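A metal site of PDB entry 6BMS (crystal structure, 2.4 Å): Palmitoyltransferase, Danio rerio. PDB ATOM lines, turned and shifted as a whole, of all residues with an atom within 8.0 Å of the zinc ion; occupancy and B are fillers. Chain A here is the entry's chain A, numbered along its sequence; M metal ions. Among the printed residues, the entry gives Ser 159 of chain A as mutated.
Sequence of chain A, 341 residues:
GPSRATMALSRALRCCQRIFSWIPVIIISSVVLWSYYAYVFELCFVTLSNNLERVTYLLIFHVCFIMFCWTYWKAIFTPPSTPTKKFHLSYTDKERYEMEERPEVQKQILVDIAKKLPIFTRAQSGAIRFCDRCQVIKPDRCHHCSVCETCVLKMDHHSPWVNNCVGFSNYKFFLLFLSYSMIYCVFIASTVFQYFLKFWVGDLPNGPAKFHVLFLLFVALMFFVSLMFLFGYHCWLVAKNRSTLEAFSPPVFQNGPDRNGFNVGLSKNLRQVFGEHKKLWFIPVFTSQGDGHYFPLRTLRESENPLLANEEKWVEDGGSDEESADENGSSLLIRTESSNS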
ATOM      1  N   PRO A  80       9.261  26.615  -7.035  1.00  0.00           N
ATOM      2  CA  PRO A  80      10.572  26.625  -7.695  1.00  0.00           C
ATOM      3  C   PRO A  80      11.636  27.276  -6.830  1.00  0.00           C
ATOM      4  O   PRO A  80      11.378  28.183  -6.036  1.00  0.00           O
ATOM      5  CB  PRO A  80      10.325  27.452  -8.965  1.00  0.00           C
ATOM      6  CG  PRO A  80       9.085  28.242  -8.675  1.00  0.00           C
ATOM      7  CD  PRO A  80       8.256  27.380  -7.785  1.00  0.00           C
ATOM      8  N   HIS A 143      15.826  29.977 -15.964  1.00  0.00           N
ATOM      9  CA  HIS A 143      15.011  30.651 -16.976  1.00  0.00           C
ATOM     10  C   HIS A 143      13.806  31.301 -16.319  1.00  0.00           C
ATOM     11  O   HIS A 143      13.383  30.889 -15.240  1.00  0.00           O
ATOM     12  CB  HIS A 143      14.561  29.684 -18.083  1.00  0.00           C
ATOM     13  CG  HIS A 143      15.694  29.021 -18.804  1.00  0.00           C
ATOM     14  ND1 HIS A 143      16.128  29.433 -20.042  1.00  0.00           N
ATOM     15  CD2 HIS A 143      16.481  27.979 -18.456  1.00  0.00           C
ATOM     16  CE1 HIS A 143      17.139  28.676 -20.431  1.00  0.00           C
ATOM     17  NE2 HIS A 143      17.367  27.782 -19.485  1.00  0.00           N
ATOM     18  N   HIS A 144      13.260  32.315 -16.979  1.00  0.00           N
ATOM     19  CA  HIS A 144      12.093  32.998 -16.443  1.00  0.00           C
ATOM     20  C   HIS A 144      10.820  32.294 -16.894  1.00  0.00           C
ATOM     21  O   HIS A 144      10.641  31.992 -18.077  1.00  0.00           O
ATOM     22  CB  HIS A 144      12.066  34.463 -16.890  1.00  0.00           C
ATOM     23  CG  HIS A 144      11.034  35.291 -16.193  1.00  0.00           C
ATOM     24  ND1 HIS A 144      10.906  35.332 -14.817  1.00  0.00           N
ATOM     25  CD2 HIS A 144      10.064  36.101 -16.686  1.00  0.00           C
ATOM     26  CE1 HIS A 144       9.919  36.146 -14.495  1.00  0.00           C
ATOM     27  NE2 HIS A 144       9.378  36.618 -15.603  1.00  0.00           N
ATOM     28  N   CYS A 145       9.945  32.001 -15.936  1.00  0.00           N
ATOM     29  CA  CYS A 145       8.619  31.465 -16.229  1.00  0.00           C
ATOM     30  C   CYS A 145       7.596  32.585 -16.097  1.00  0.00           C
ATOM     31  O   CYS A 145       7.423  33.148 -15.008  1.00  0.00           O
ATOM     32  CB  CYS A 145       8.250  30.318 -15.292  1.00  0.00           C
ATOM     33  SG  CYS A 145       6.585  29.696 -15.606  1.00  0.00           S
ATOM     34  N   SER A 146       6.917  32.890 -17.205  1.00  0.00           N
ATOM     35  CA  SER A 146       5.908  33.943 -17.186  1.00  0.00           C
ATOM     36  C   SER A 146       4.623  33.493 -16.499  1.00  0.00           C
ATOM     37  O   SER A 146       3.839  34.346 -16.060  1.00  0.00           O
ATOM     38  CB  SER A 146       5.596  34.399 -18.618  1.00  0.00           C
ATOM     39  OG  SER A 146       4.957  33.360 -19.342  1.00  0.00           O
ATOM     40  N   VAL A 147       4.384  32.183 -16.384  1.00  0.00           N
ATOM     41  CA  VAL A 147       3.223  31.710 -15.627  1.00  0.00           C
ATOM     42  C   VAL A 147       3.482  31.851 -14.136  1.00  0.00           C
ATOM     43  O   VAL A 147       2.742  32.539 -13.421  1.00  0.00           O
ATOM     44  CB  VAL A 147       2.882  30.270 -16.021  1.00  0.00           C
ATOM     45  CG1 VAL A 147       1.568  29.862 -15.372  1.00  0.00           C
ATOM     46  CG2 VAL A 147       2.795  30.127 -17.528  1.00  0.00           C
ATOM     47  N   CYS A 148       4.541  31.198 -13.642  1.00  0.00           N
ATOM     48  CA  CYS A 148       4.996  31.448 -12.281  1.00  0.00           C
ATOM     49  C   CYS A 148       5.518  32.869 -12.100  1.00  0.00           C
ATOM     50  O   CYS A 148       5.648  33.311 -10.952  1.00  0.00           O
ATOM     51  CB  CYS A 148       6.094  30.442 -11.901  1.00  0.00           C
ATOM     52  SG  CYS A 148       5.615  28.709 -12.022  1.00  0.00           S
ATOM     53  N   GLU A 149       5.809  33.578 -13.184  1.00  0.00           N
ATOM     54  CA  GLU A 149       6.280  34.963 -13.159  1.00  0.00           C
ATOM     55  C   GLU A 149       7.534  35.107 -12.318  1.00  0.00           C
ATOM     56  O   GLU A 149       7.726  36.091 -11.596  1.00  0.00           O
ATOM     57  CB  GLU A 149       5.191  35.915 -12.638  1.00  0.00           C
ATOM     58  CG  GLU A 149       3.841  35.772 -13.314  1.00  0.00           C
ATOM     59  CD  GLU A 149       2.762  36.514 -12.551  1.00  0.00           C
ATOM     60  OE1 GLU A 149       2.411  37.640 -12.957  1.00  0.00           O
ATOM     61  OE2 GLU A 149       2.254  35.965 -11.547  1.00  0.00           O
ATOM     62  N   THR A 150       8.428  34.121 -12.420  1.00  0.00           N
ATOM     63  CA  THR A 150       9.662  34.187 -11.645  1.00  0.00           C
ATOM     64  C   THR A 150      10.754  33.411 -12.356  1.00  0.00           C
ATOM     65  O   THR A 150      10.491  32.471 -13.118  1.00  0.00           O
ATOM     66  CB  THR A 150       9.491  33.656 -10.215  1.00  0.00           C
ATOM     67  OG1 THR A 150      10.709  33.869  -9.494  1.00  0.00           O
ATOM     68  CG2 THR A 150       9.176  32.171 -10.233  1.00  0.00           C
ATOM     69  N   VAL A 152      13.478  30.672 -12.444  1.00  0.00           N
ATOM     70  CA  VAL A 152      13.418  29.316 -11.912  1.00  0.00           C
ATOM     71  C   VAL A 152      14.735  28.632 -12.233  1.00  0.00           C
ATOM     72  O   VAL A 152      15.199  28.663 -13.382  1.00  0.00           O
ATOM     73  CB  VAL A 152      12.221  28.524 -12.503  1.00  0.00           C
ATOM     74  CG1 VAL A 152      12.300  27.058 -12.125  1.00  0.00           C
ATOM     75  CG2 VAL A 152      10.887  29.146 -12.072  1.00  0.00           C
ATOM     76  N   MET A 155      15.199  25.256 -14.736  1.00  0.00           N
ATOM     77  CA  MET A 155      13.819  25.063 -15.163  1.00  0.00           C
ATOM     78  C   MET A 155      13.764  24.056 -16.296  1.00  0.00           C
ATOM     79  O   MET A 155      14.314  24.293 -17.378  1.00  0.00           O
ATOM     80  CB  MET A 155      13.194  26.375 -15.598  1.00  0.00           C
ATOM     81  CG  MET A 155      11.726  26.231 -15.951  1.00  0.00           C
ATOM     82  SD  MET A 155      11.188  27.438 -17.172  1.00  0.00           S
ATOM     83  CE  MET A 155      11.264  28.918 -16.171  1.00  0.00           C
ATOM     84  N   HIS A 157      10.557  22.838 -17.423  1.00  0.00           N
ATOM     85  CA  HIS A 157       9.439  23.387 -18.180  1.00  0.00           C
ATOM     86  C   HIS A 157       8.288  23.660 -17.230  1.00  0.00           C
ATOM     87  O   HIS A 157       8.189  23.054 -16.162  1.00  0.00           O
ATOM     88  CB  HIS A 157       8.966  22.427 -19.287  1.00  0.00           C
ATOM     89  CG  HIS A 157       8.250  21.219 -18.764  1.00  0.00           C
ATOM     90  ND1 HIS A 157       8.918  20.138 -18.231  1.00  0.00           N
ATOM     91  CD2 HIS A 157       6.928  20.925 -18.694  1.00  0.00           C
ATOM     92  CE1 HIS A 157       8.038  19.224 -17.860  1.00  0.00           C
ATOM     93  NE2 HIS A 157       6.829  19.678 -18.122  1.00  0.00           N
ATOM     94  N   HIS A 158       7.403  24.566 -17.633  1.00  0.00           N
ATOM     95  CA  HIS A 158       6.184  24.794 -16.864  1.00  0.00           C
ATOM     96  C   HIS A 158       5.126  23.777 -17.270  1.00  0.00           C
ATOM     97  O   HIS A 158       4.801  23.646 -18.454  1.00  0.00           O
ATOM     98  CB  HIS A 158       5.653  26.212 -17.063  1.00  0.00           C
ATOM     99  CG  HIS A 158       4.457  26.502 -16.214  1.00  0.00           C
ATOM    100  ND1 HIS A 158       4.547  26.738 -14.855  1.00  0.00           N
ATOM    101  CD2 HIS A 158       3.140  26.536 -16.521  1.00  0.00           C
ATOM    102  CE1 HIS A 158       3.336  26.933 -14.373  1.00  0.00           C
ATOM    103  NE2 HIS A 158       2.462  26.815 -15.352  1.00  0.00           N
ATOM    104  N   SER A 159       4.585  23.070 -16.285  1.00  0.00           N
ATOM    105  CA  SER A 159       3.655  21.978 -16.536  1.00  0.00           C
ATOM    106  C   SER A 159       2.243  22.385 -16.138  1.00  0.00           C
ATOM    107  O   SER A 159       1.991  22.642 -14.946  1.00  0.00           O
ATOM    108  CB  SER A 159       4.098  20.733 -15.770  1.00  0.00           C
ATOM    109  OG  SER A 159       3.151  19.687 -15.920  1.00  0.00           O
ATOM    110  N   PRO A 160       1.314  22.469 -17.083  1.00  0.00           N
ATOM    111  CA  PRO A 160      -0.098  22.648 -16.720  1.00  0.00           C
ATOM    112  C   PRO A 160      -0.646  21.469 -15.947  1.00  0.00           C
ATOM    113  O   PRO A 160      -1.600  21.626 -15.177  1.00  0.00           O
ATOM    114  CB  PRO A 160      -0.804  22.805 -18.074  1.00  0.00           C
ATOM    115  CG  PRO A 160       0.284  23.105 -19.065  1.00  0.00           C
ATOM    116  CD  PRO A 160       1.508  22.418 -18.543  1.00  0.00           C
ATOM    117  N   ASN A 163       0.234  22.003 -12.622  1.00  0.00           N
ATOM    118  CA  ASN A 163      -0.064  23.412 -12.350  1.00  0.00           C
ATOM    119  C   ASN A 163       1.127  24.083 -11.681  1.00  0.00           C
ATOM    120  O   ASN A 163       1.005  24.799 -10.688  1.00  0.00           O
ATOM    121  CB  ASN A 163      -1.330  23.551 -11.499  1.00  0.00           C
ATOM    122  CG  ASN A 163      -1.819  24.982 -11.418  1.00  0.00           C
ATOM    123  OD1 ASN A 163      -1.413  25.839 -12.212  1.00  0.00           O
ATOM    124  ND2 ASN A 163      -2.706  25.250 -10.463  1.00  0.00           N
ATOM    125  N   ASN A 164       2.313  23.821 -12.214  1.00  0.00           N
ATOM    126  CA  ASN A 164       3.515  24.225 -11.501  1.00  0.00           C
ATOM    127  C   ASN A 164       4.703  24.105 -12.441  1.00  0.00           C
ATOM    128  O   ASN A 164       4.663  23.364 -13.422  1.00  0.00           O
ATOM    129  CB  ASN A 164       3.722  23.364 -10.248  1.00  0.00           C
ATOM    130  CG  ASN A 164       4.834  23.883  -9.354  1.00  0.00           C
ATOM    131  OD1 ASN A 164       5.191  25.056  -9.414  1.00  0.00           O
ATOM    132  ND2 ASN A 164       5.377  23.006  -8.524  1.00  0.00           N
ATOM    133  N   CYS A 165       5.760  24.849 -12.115  1.00  0.00           N
ATOM    134  CA  CYS A 165       7.020  24.660 -12.809  1.00  0.00           C
ATOM    135  C   CYS A 165       7.679  23.345 -12.386  1.00  0.00           C
ATOM    136  O   CYS A 165       7.573  22.905 -11.243  1.00  0.00           O
ATOM    137  CB  CYS A 165       7.981  25.821 -12.557  1.00  0.00           C
ATOM    138  SG  CYS A 165       8.026  27.061 -13.877  1.00  0.00           S
ATOM    139  N   VAL A 166       8.339  22.716 -13.341  1.00  0.00           N
ATOM    140  CA  VAL A 166       9.194  21.562 -13.095  1.00  0.00           C
ATOM    141  C   VAL A 166      10.630  22.013 -13.344  1.00  0.00           C
ATOM    142  O   VAL A 166      10.982  22.402 -14.469  1.00  0.00           O
ATOM    143  CB  VAL A 166       8.815  20.363 -13.973  1.00  0.00           C
ATOM    144  CG1 VAL A 166       9.792  19.225 -13.722  1.00  0.00           C
ATOM    145  CG2 VAL A 166       7.390  19.924 -13.678  1.00  0.00           C
HETATM  146 ZN    ZN M   1       6.214  27.985 -14.170  1.00  0.00          ZN
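The backbone NH (N) of Val 147 lies close to the side-chain sulfur (SG) of Cys 145, at 3.4 Å. The backbone carbonyl oxygen of Thr 150 is in hydrogen-bond range of the backbone NH of Cys 145, 2.9 Å away.
The side-chain sulfur (SG) of Cys 165 is bound to the zinc ion, at 2.1 Å. The zinc ion is bound by ND1 of His 158, at 2.2 Å. The side-chain sulfur (SG) of Cys 145 is bound to the zinc ion (2.3 Å). SG of Cys 148 binds the zinc ion, at 2.3 Å.
Four residues have an atom within 4 Å of the zinc ion: Cys 145, Cys 148, His 158 and Cys 165.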
